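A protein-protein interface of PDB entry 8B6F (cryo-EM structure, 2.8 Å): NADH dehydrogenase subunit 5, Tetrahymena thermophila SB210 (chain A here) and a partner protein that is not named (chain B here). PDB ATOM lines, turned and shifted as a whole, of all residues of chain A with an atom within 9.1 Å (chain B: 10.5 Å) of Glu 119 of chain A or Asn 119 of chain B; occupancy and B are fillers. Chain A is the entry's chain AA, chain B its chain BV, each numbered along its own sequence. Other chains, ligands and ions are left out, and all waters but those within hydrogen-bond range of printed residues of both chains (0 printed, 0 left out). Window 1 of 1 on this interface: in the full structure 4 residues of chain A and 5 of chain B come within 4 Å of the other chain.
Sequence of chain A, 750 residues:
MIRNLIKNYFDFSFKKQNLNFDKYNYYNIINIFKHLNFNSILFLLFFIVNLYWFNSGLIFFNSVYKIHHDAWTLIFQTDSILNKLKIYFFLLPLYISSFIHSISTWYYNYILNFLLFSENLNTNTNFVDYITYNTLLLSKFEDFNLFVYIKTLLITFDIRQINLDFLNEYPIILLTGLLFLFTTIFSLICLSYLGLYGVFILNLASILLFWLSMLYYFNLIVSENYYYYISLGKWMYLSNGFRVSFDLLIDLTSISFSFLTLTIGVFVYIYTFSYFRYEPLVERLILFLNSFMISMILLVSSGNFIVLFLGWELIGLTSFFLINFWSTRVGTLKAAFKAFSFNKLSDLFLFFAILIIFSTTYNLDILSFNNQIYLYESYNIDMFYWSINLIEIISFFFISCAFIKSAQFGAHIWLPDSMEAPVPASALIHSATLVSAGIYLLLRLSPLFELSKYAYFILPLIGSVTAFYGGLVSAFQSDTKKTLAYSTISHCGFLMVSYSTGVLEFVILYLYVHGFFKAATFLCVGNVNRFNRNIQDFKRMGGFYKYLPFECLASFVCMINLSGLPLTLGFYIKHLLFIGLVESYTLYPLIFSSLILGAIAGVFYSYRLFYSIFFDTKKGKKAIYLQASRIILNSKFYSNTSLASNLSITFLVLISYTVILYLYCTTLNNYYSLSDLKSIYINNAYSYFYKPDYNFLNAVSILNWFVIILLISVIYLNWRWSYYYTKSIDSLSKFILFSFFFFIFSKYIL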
ATOM      1  N   ASN A 109     -13.805  29.885   8.843  1.00  0.00           N
ATOM      2  CA  ASN A 109     -12.567  29.147   9.060  1.00  0.00           C
ATOM      3  C   ASN A 109     -11.398  30.098   9.282  1.00  0.00           C
ATOM      4  O   ASN A 109     -10.533  29.845  10.127  1.00  0.00           O
ATOM      5  CB  ASN A 109     -12.292  28.218   7.879  1.00  0.00           C
ATOM      6  CG  ASN A 109     -13.391  27.193   7.680  1.00  0.00           C
ATOM      7  OD1 ASN A 109     -14.089  26.825   8.623  1.00  0.00           O
ATOM      8  ND2 ASN A 109     -13.547  26.726   6.448  1.00  0.00           N
ATOM      9  N   TYR A 110     -11.349  31.194   8.524  1.00  0.00           N
ATOM     10  CA  TYR A 110     -10.306  32.189   8.742  1.00  0.00           C
ATOM     11  C   TYR A 110     -10.392  32.773  10.146  1.00  0.00           C
ATOM     12  O   TYR A 110      -9.368  32.946  10.815  1.00  0.00           O
ATOM     13  CB  TYR A 110     -10.404  33.304   7.702  1.00  0.00           C
ATOM     14  CG  TYR A 110      -9.737  34.581   8.158  1.00  0.00           C
ATOM     15  CD1 TYR A 110      -8.354  34.687   8.207  1.00  0.00           C
ATOM     16  CD2 TYR A 110     -10.494  35.674   8.559  1.00  0.00           C
ATOM     17  CE1 TYR A 110      -7.742  35.851   8.634  1.00  0.00           C
ATOM     18  CE2 TYR A 110      -9.893  36.840   8.985  1.00  0.00           C
ATOM     19  CZ  TYR A 110      -8.518  36.923   9.020  1.00  0.00           C
ATOM     20  OH  TYR A 110      -7.921  38.084   9.448  1.00  0.00           O
ATOM     21  N   LEU A 112     -11.662  31.374  12.848  1.00  0.00           N
ATOM     22  CA  LEU A 112     -11.241  30.375  13.823  1.00  0.00           C
ATOM     23  C   LEU A 112      -9.727  30.227  13.840  1.00  0.00           C
ATOM     24  O   LEU A 112      -9.117  30.143  14.912  1.00  0.00           O
ATOM     25  CB  LEU A 112     -11.899  29.029  13.524  1.00  0.00           C
ATOM     26  CG  LEU A 112     -13.419  28.930  13.670  1.00  0.00           C
ATOM     27  CD1 LEU A 112     -13.828  27.469  13.742  1.00  0.00           C
ATOM     28  CD2 LEU A 112     -13.935  29.716  14.856  1.00  0.00           C
ATOM     29  N   ASN A 113      -9.100  30.183  12.665  1.00  0.00           N
ATOM     30  CA  ASN A 113      -7.647  30.091  12.622  1.00  0.00           C
ATOM     31  C   ASN A 113      -7.009  31.317  13.256  1.00  0.00           C
ATOM     32  O   ASN A 113      -6.027  31.205  13.999  1.00  0.00           O
ATOM     33  CB  ASN A 113      -7.174  29.929  11.179  1.00  0.00           C
ATOM     34  CG  ASN A 113      -7.671  28.650  10.546  1.00  0.00           C
ATOM     35  OD1 ASN A 113      -8.568  27.991  11.071  1.00  0.00           O
ATOM     36  ND2 ASN A 113      -7.094  28.294   9.406  1.00  0.00           N
ATOM     37  N   PHE A 114      -7.553  32.502  12.970  1.00  0.00           N
ATOM     38  CA  PHE A 114      -7.011  33.724  13.551  1.00  0.00           C
ATOM     39  C   PHE A 114      -7.102  33.698  15.070  1.00  0.00           C
ATOM     40  O   PHE A 114      -6.150  34.074  15.764  1.00  0.00           O
ATOM     41  CB  PHE A 114      -7.757  34.936  12.987  1.00  0.00           C
ATOM     42  CG  PHE A 114      -7.363  36.242  13.617  1.00  0.00           C
ATOM     43  CD1 PHE A 114      -8.034  36.724  14.728  1.00  0.00           C
ATOM     44  CD2 PHE A 114      -6.331  36.997  13.084  1.00  0.00           C
ATOM     45  CE1 PHE A 114      -7.675  37.928  15.304  1.00  0.00           C
ATOM     46  CE2 PHE A 114      -5.968  38.203  13.655  1.00  0.00           C
ATOM     47  CZ  PHE A 114      -6.640  38.667  14.766  1.00  0.00           C
ATOM     48  N   LEU A 116      -7.494  31.024  17.175  1.00  0.00           N
ATOM     49  CA  LEU A 116      -6.958  29.866  17.876  1.00  0.00           C
ATOM     50  C   LEU A 116      -5.552  29.482  17.440  1.00  0.00           C
ATOM     51  O   LEU A 116      -5.000  28.518  17.977  1.00  0.00           O
ATOM     52  CB  LEU A 116      -7.900  28.669  17.691  1.00  0.00           C
ATOM     53  CG  LEU A 116      -9.098  28.581  18.644  1.00  0.00           C
ATOM     54  CD1 LEU A 116      -9.725  29.941  18.907  1.00  0.00           C
ATOM     55  CD2 LEU A 116     -10.142  27.633  18.084  1.00  0.00           C
ATOM     56  N   PHE A 117      -4.953  30.205  16.495  1.00  0.00           N
ATOM     57  CA  PHE A 117      -3.594  29.908  16.041  1.00  0.00           C
ATOM     58  C   PHE A 117      -3.468  28.447  15.624  1.00  0.00           C
ATOM     59  O   PHE A 117      -2.450  27.797  15.869  1.00  0.00           O
ATOM     60  CB  PHE A 117      -2.571  30.232  17.132  1.00  0.00           C
ATOM     61  CG  PHE A 117      -2.444  31.694  17.443  1.00  0.00           C
ATOM     62  CD1 PHE A 117      -3.478  32.378  18.059  1.00  0.00           C
ATOM     63  CD2 PHE A 117      -1.275  32.375  17.156  1.00  0.00           C
ATOM     64  CE1 PHE A 117      -3.359  33.720  18.358  1.00  0.00           C
ATOM     65  CE2 PHE A 117      -1.148  33.716  17.453  1.00  0.00           C
ATOM     66  CZ  PHE A 117      -2.193  34.389  18.057  1.00  0.00           C
ATOM     67  N   SER A 118      -4.507  27.919  14.983  1.00  0.00           N
ATOM     68  CA  SER A 118      -4.643  26.484  14.779  1.00  0.00           C
ATOM     69  C   SER A 118      -4.798  26.151  13.303  1.00  0.00           C
ATOM     70  O   SER A 118      -5.654  26.720  12.619  1.00  0.00           O
ATOM     71  CB  SER A 118      -5.842  25.938  15.560  1.00  0.00           C
ATOM     72  OG  SER A 118      -7.049  26.545  15.133  1.00  0.00           O
ATOM     73  N   GLU A 119      -3.966  25.222  12.830  1.00  0.00           N
ATOM     74  CA  GLU A 119      -4.144  24.539  11.552  1.00  0.00           C
ATOM     75  C   GLU A 119      -4.523  25.468  10.404  1.00  0.00           C
ATOM     76  O   GLU A 119      -4.307  26.682  10.473  1.00  0.00           O
ATOM     77  CB  GLU A 119      -5.208  23.442  11.703  1.00  0.00           C
ATOM     78  CG  GLU A 119      -6.633  23.957  11.902  1.00  0.00           C
ATOM     79  CD  GLU A 119      -7.652  22.838  11.958  1.00  0.00           C
ATOM     80  OE1 GLU A 119      -7.240  21.660  11.975  1.00  0.00           O
ATOM     81  OE2 GLU A 119      -8.864  23.136  11.983  1.00  0.00           O
ATOM     82  N   ASN A 120      -5.069  24.891   9.338  1.00  0.00           N
ATOM     83  CA  ASN A 120      -5.556  25.616   8.174  1.00  0.00           C
ATOM     84  C   ASN A 120      -7.039  25.297   7.986  1.00  0.00           C
ATOM     85  O   ASN A 120      -7.682  24.695   8.850  1.00  0.00           O
ATOM     86  CB  ASN A 120      -4.740  25.248   6.933  1.00  0.00           C
ATOM     87  CG  ASN A 120      -3.246  25.278   7.187  1.00  0.00           C
ATOM     88  OD1 ASN A 120      -2.763  26.032   8.031  1.00  0.00           O
ATOM     89  ND2 ASN A 120      -2.506  24.451   6.456  1.00  0.00           N
ATOM     90  N   LEU A 121      -7.583  25.705   6.839  1.00  0.00           N
ATOM     91  CA  LEU A 121      -8.967  25.390   6.485  1.00  0.00           C
ATOM     92  C   LEU A 121      -9.031  23.928   6.040  1.00  0.00           C
ATOM     93  O   LEU A 121      -9.238  23.600   4.871  1.00  0.00           O
ATOM     94  CB  LEU A 121      -9.478  26.330   5.401  1.00  0.00           C
ATOM     95  CG  LEU A 121      -9.486  27.836   5.696  1.00  0.00           C
ATOM     96  CD1 LEU A 121      -8.102  28.471   5.558  1.00  0.00           C
ATOM     97  CD2 LEU A 121     -10.483  28.543   4.795  1.00  0.00           C
ATOM     98  N   ASN A 122      -8.835  23.041   7.016  1.00  0.00           N
ATOM     99  CA  ASN A 122      -8.688  21.614   6.756  1.00  0.00           C
ATOM    100  C   ASN A 122      -7.411  21.383   5.957  1.00  0.00           C
ATOM    101  O   ASN A 122      -6.464  20.763   6.451  1.00  0.00           O
ATOM    102  CB  ASN A 122      -9.908  21.058   6.016  1.00  0.00           C
ATOM    103  CG  ASN A 122      -9.874  19.548   5.892  1.00  0.00           C
ATOM    104  OD1 ASN A 122      -9.319  19.004   4.937  1.00  0.00           O
ATOM    105  ND2 ASN A 122     -10.468  18.861   6.862  1.00  0.00           N
ATOM    106  N   THR A 123      -7.380  21.881   4.727  1.00  0.00           N
ATOM    107  CA  THR A 123      -6.199  21.877   3.877  1.00  0.00           C
ATOM    108  C   THR A 123      -5.796  23.319   3.571  1.00  0.00           C
ATOM    109  O   THR A 123      -6.431  24.274   4.022  1.00  0.00           O
ATOM    110  CB  THR A 123      -6.458  21.087   2.591  1.00  0.00           C
ATOM    111  OG1 THR A 123      -7.701  21.501   2.011  1.00  0.00           O
ATOM    112  CG2 THR A 123      -6.509  19.595   2.882  1.00  0.00           C
ATOM    113  N   ASN A 124      -4.728  23.470   2.787  1.00  0.00           N
ATOM    114  CA  ASN A 124      -4.198  24.778   2.417  1.00  0.00           C
ATOM    115  C   ASN A 124      -4.726  25.258   1.068  1.00  0.00           C
ATOM    116  O   ASN A 124      -4.026  25.975   0.346  1.00  0.00           O
ATOM    117  CB  ASN A 124      -2.669  24.743   2.407  1.00  0.00           C
ATOM    118  CG  ASN A 124      -2.114  23.803   1.356  1.00  0.00           C
ATOM    119  OD1 ASN A 124      -2.647  22.715   1.134  1.00  0.00           O
ATOM    120  ND2 ASN A 124      -1.036  24.219   0.702  1.00  0.00           N
ATOM    121  N   LEU B  50       9.852  32.748  20.306  1.00  0.00           N
ATOM    122  CA  LEU B  50       8.398  32.849  20.301  1.00  0.00           C
ATOM    123  C   LEU B  50       7.885  33.379  21.631  1.00  0.00           C
ATOM    124  O   LEU B  50       6.943  34.180  21.669  1.00  0.00           O
ATOM    125  CB  LEU B  50       7.780  31.486  19.993  1.00  0.00           C
ATOM    126  CG  LEU B  50       7.964  30.975  18.563  1.00  0.00           C
ATOM    127  CD1 LEU B  50       7.487  29.540  18.455  1.00  0.00           C
ATOM    128  CD2 LEU B  50       7.229  31.857  17.569  1.00  0.00           C
ATOM    129  N   ASP B  54       5.770  36.773  21.998  1.00  0.00           N
ATOM    130  CA  ASP B  54       4.432  36.738  22.577  1.00  0.00           C
ATOM    131  C   ASP B  54       4.318  37.690  23.759  1.00  0.00           C
ATOM    132  O   ASP B  54       3.315  38.399  23.897  1.00  0.00           O
ATOM    133  CB  ASP B  54       4.079  35.313  23.000  1.00  0.00           C
ATOM    134  CG  ASP B  54       3.912  34.377  21.818  1.00  0.00           C
ATOM    135  OD1 ASP B  54       4.023  34.845  20.665  1.00  0.00           O
ATOM    136  OD2 ASP B  54       3.665  33.173  22.041  1.00  0.00           O
ATOM    137  N   ARG B 112      -4.039  32.769  25.562  1.00  0.00           N
ATOM    138  CA  ARG B 112      -4.726  31.484  25.490  1.00  0.00           C
ATOM    139  C   ARG B 112      -4.044  30.541  24.510  1.00  0.00           C
ATOM    140  O   ARG B 112      -4.053  29.323  24.713  1.00  0.00           O
ATOM    141  CB  ARG B 112      -6.189  31.702  25.096  1.00  0.00           C
ATOM    142  CG  ARG B 112      -6.991  30.428  24.851  1.00  0.00           C
ATOM    143  CD  ARG B 112      -7.022  29.544  26.083  1.00  0.00           C
ATOM    144  NE  ARG B 112      -8.010  28.477  25.983  1.00  0.00           N
ATOM    145  CZ  ARG B 112      -9.301  28.618  26.248  1.00  0.00           C
ATOM    146  NH1 ARG B 112      -9.809  29.782  26.616  1.00  0.00           N
ATOM    147  NH2 ARG B 112     -10.103  27.563  26.145  1.00  0.00           N
ATOM    148  N   ASN B 113      -3.457  31.083  23.444  1.00  0.00           N
ATOM    149  CA  ASN B 113      -2.850  30.244  22.419  1.00  0.00           C
ATOM    150  C   ASN B 113      -1.756  29.358  22.998  1.00  0.00           C
ATOM    151  O   ASN B 113      -1.643  28.181  22.639  1.00  0.00           O
ATOM    152  CB  ASN B 113      -2.286  31.125  21.305  1.00  0.00           C
ATOM    153  CG  ASN B 113      -1.267  30.403  20.452  1.00  0.00           C
ATOM    154  OD1 ASN B 113      -1.437  29.232  20.121  1.00  0.00           O
ATOM    155  ND2 ASN B 113      -0.190  31.098  20.103  1.00  0.00           N
ATOM    156  N   ALA B 114      -0.933  29.908  23.888  1.00  0.00           N
ATOM    157  CA  ALA B 114       0.190  29.151  24.428  1.00  0.00           C
ATOM    158  C   ALA B 114      -0.277  27.953  25.245  1.00  0.00           C
ATOM    159  O   ALA B 114       0.220  26.836  25.068  1.00  0.00           O
ATOM    160  CB  ALA B 114       1.066  30.066  25.276  1.00  0.00           C
ATOM    161  N   ILE B 115      -1.230  28.166  26.153  1.00  0.00           N
ATOM    162  CA  ILE B 115      -1.707  27.059  26.975  1.00  0.00           C
ATOM    163  C   ILE B 115      -2.447  26.030  26.128  1.00  0.00           C
ATOM    164  O   ILE B 115      -2.370  24.827  26.400  1.00  0.00           O
ATOM    165  CB  ILE B 115      -2.579  27.584  28.133  1.00  0.00           C
ATOM    166  CG1 ILE B 115      -3.823  28.305  27.604  1.00  0.00           C
ATOM    167  CG2 ILE B 115      -1.754  28.507  29.021  1.00  0.00           C
ATOM    168  CD1 ILE B 115      -4.765  28.786  28.698  1.00  0.00           C
ATOM    169  N   THR B 116      -3.166  26.469  25.098  1.00  0.00           N
ATOM    170  CA  THR B 116      -3.880  25.551  24.216  1.00  0.00           C
ATOM    171  C   THR B 116      -2.911  25.008  23.175  1.00  0.00           C
ATOM    172  O   THR B 116      -2.496  25.730  22.264  1.00  0.00           O
ATOM    173  CB  THR B 116      -5.057  26.251  23.543  1.00  0.00           C
ATOM    174  OG1 THR B 116      -4.714  27.615  23.263  1.00  0.00           O
ATOM    175  CG2 THR B 116      -6.283  26.202  24.431  1.00  0.00           C
ATOM    176  N   ALA B 117      -2.558  23.732  23.303  1.00  0.00           N
ATOM    177  CA  ALA B 117      -1.635  23.084  22.376  1.00  0.00           C
ATOM    178  C   ALA B 117      -2.425  22.357  21.289  1.00  0.00           C
ATOM    179  O   ALA B 117      -2.546  21.131  21.265  1.00  0.00           O
ATOM    180  CB  ALA B 117      -0.709  22.137  23.131  1.00  0.00           C
ATOM    181  N   HIS B 118      -2.973  23.156  20.373  1.00  0.00           N
ATOM    182  CA  HIS B 118      -3.729  22.602  19.258  1.00  0.00           C
ATOM    183  C   HIS B 118      -2.820  22.017  18.185  1.00  0.00           C
ATOM    184  O   HIS B 118      -3.187  21.030  17.539  1.00  0.00           O
ATOM    185  CB  HIS B 118      -4.620  23.680  18.639  1.00  0.00           C
ATOM    186  CG  HIS B 118      -5.643  24.232  19.582  1.00  0.00           C
ATOM    187  ND1 HIS B 118      -6.126  23.521  20.659  1.00  0.00           N
ATOM    188  CD2 HIS B 118      -6.273  25.429  19.611  1.00  0.00           C
ATOM    189  CE1 HIS B 118      -7.013  24.254  21.307  1.00  0.00           C
ATOM    190  NE2 HIS B 118      -7.120  25.417  20.693  1.00  0.00           N
ATOM    191  N   ASN B 119      -1.640  22.604  17.982  1.00  0.00           N
ATOM    192  CA  ASN B 119      -0.736  22.184  16.911  1.00  0.00           C
ATOM    193  C   ASN B 119       0.062  20.962  17.367  1.00  0.00           C
ATOM    194  O   ASN B 119       1.280  20.994  17.553  1.00  0.00           O
ATOM    195  CB  ASN B 119       0.177  23.332  16.511  1.00  0.00           C
ATOM    196  CG  ASN B 119      -0.594  24.545  16.032  1.00  0.00           C
ATOM    197  OD1 ASN B 119      -0.956  24.641  14.859  1.00  0.00           O
ATOM    198  ND2 ASN B 119      -0.850  25.479  16.939  1.00  0.00           N
ATOM    199  N   PHE B 120      -0.663  19.863  17.547  1.00  0.00           N
ATOM    200  CA  PHE B 120      -0.085  18.568  17.876  1.00  0.00           C
ATOM    201  C   PHE B 120      -0.404  17.615  16.735  1.00  0.00           C
ATOM    202  O   PHE B 120      -1.554  17.536  16.295  1.00  0.00           O
ATOM    203  CB  PHE B 120      -0.639  18.045  19.202  1.00  0.00           C
ATOM    204  CG  PHE B 120       0.189  16.958  19.821  1.00  0.00           C
ATOM    205  CD1 PHE B 120       1.274  17.268  20.623  1.00  0.00           C
ATOM    206  CD2 PHE B 120      -0.127  15.629  19.617  1.00  0.00           C
ATOM    207  CE1 PHE B 120       2.032  16.271  21.198  1.00  0.00           C
ATOM    208  CE2 PHE B 120       0.626  14.630  20.188  1.00  0.00           C
ATOM    209  CZ  PHE B 120       1.706  14.950  20.978  1.00  0.00           C
ATOM    210  N   GLY B 121       0.609  16.900  16.252  1.00  0.00           N
ATOM    211  CA  GLY B 121       0.444  16.127  15.033  1.00  0.00           C
ATOM    212  C   GLY B 121      -0.361  14.855  15.189  1.00  0.00           C
ATOM    213  O   GLY B 121      -0.652  14.205  14.178  1.00  0.00           O
ATOM    214  N   TRP B 122      -0.735  14.489  16.411  1.00  0.00           N
ATOM    215  CA  TRP B 122      -1.425  13.229  16.656  1.00  0.00           C
ATOM    216  C   TRP B 122      -2.923  13.307  16.397  1.00  0.00           C
ATOM    217  O   TRP B 122      -3.614  12.295  16.551  1.00  0.00           O
ATOM    218  CB  TRP B 122      -1.170  12.770  18.094  1.00  0.00           C
ATOM    219  CG  TRP B 122      -1.682  11.396  18.386  1.00  0.00           C
ATOM    220  CD1 TRP B 122      -2.776  11.071  19.132  1.00  0.00           C
ATOM    221  CD2 TRP B 122      -1.125  10.160  17.930  1.00  0.00           C
ATOM    222  NE1 TRP B 122      -2.932   9.707  19.171  1.00  0.00           N
ATOM    223  CE2 TRP B 122      -1.930   9.124  18.442  1.00  0.00           C
ATOM    224  CE3 TRP B 122      -0.021   9.828  17.141  1.00  0.00           C
ATOM    225  CZ2 TRP B 122      -1.669   7.782  18.191  1.00  0.00           C
ATOM    226  CZ3 TRP B 122       0.239   8.493  16.893  1.00  0.00           C
ATOM    227  CH2 TRP B 122      -0.581   7.486  17.417  1.00  0.00           C
ATOM    228  N   GLN B 123      -3.447  14.469  16.010  1.00  0.00           N
ATOM    229  CA  GLN B 123      -4.869  14.580  15.716  1.00  0.00           C
ATOM    230  C   GLN B 123      -5.239  13.595  14.616  1.00  0.00           C
ATOM    231  O   GLN B 123      -4.796  13.737  13.474  1.00  0.00           O
ATOM    232  CB  GLN B 123      -5.234  16.005  15.293  1.00  0.00           C
ATOM    233  CG  GLN B 123      -4.732  17.096  16.224  1.00  0.00           C
ATOM    234  CD  GLN B 123      -5.180  16.911  17.657  1.00  0.00           C
ATOM    235  OE1 GLN B 123      -6.117  16.166  17.936  1.00  0.00           O
ATOM    236  NE2 GLN B 123      -4.507  17.590  18.577  1.00  0.00           N
ATOM    237  N   ALA B 124      -6.037  12.588  14.953  1.00  0.00           N
ATOM    238  CA  ALA B 124      -6.442  11.565  13.999  1.00  0.00           C
ATOM    239  C   ALA B 124      -7.670  10.857  14.559  1.00  0.00           C
ATOM    240  O   ALA B 124      -8.265  11.300  15.547  1.00  0.00           O
ATOM    241  CB  ALA B 124      -5.290  10.594  13.721  1.00  0.00           C
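ND2 of Asn 113 of chain A is in hydrogen-bond range of O of Glu 119 of chain A (3.4 Å).
O of Asn 113 of chain B is in hydrogen-bond range of OG1 of Thr 116 of chain B.
O of Phe 117 of chain A is in hydrogen-bond range of ND2 of Asn 119 of chain B (3.0 Å).
Printed residues of chain B that touch a printed residue of chain A: Asn 113, His 118 and Asn 119.
Hydrophobic or aromatic side chains of chain B that line the printed part of chain A: His 118.
Among the printed residues, pairs that only touch across the chains: Leu 116 of chain A with His 118 of chain B, Phe 117 of chain A with Asn 113 of chain B and Glu 119 of chain A with Asn 119 of chain B.
Of chain B, only Asn 119 (3.7 Å) comes within 4 Å of Glu 119 of chain A.
No residue of chain B comes within 4 Å of Asn 113 of chain A.
No residue of chain B comes within 4 Å of Asn 120 of chain A.
Printed residues of chain B within 4 Å of Phe 117 of chain A: Asn 113 and Asn 119.
Printed residues of chain A within 4 Å of His 118 of chain B: Leu 116 (3.7 Å).
Of the printed residues of chain A, Asn 113 of chain B touches Phe 117 (3.3 Å).
Printed residues of chain B within 4 Å of Leu 116 of chain A: His 118 (3.7 Å).
Thr 123 of chain A touches none of the printed residues of chain B.
The nearest residue of chain B that does not touch Glu 119 of chain A is His 118 of chain B (6.0 Å).
The nearest printed residue of chain A that does not touch His 118 of chain B is Ser 118 of chain A (4.01 Å).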
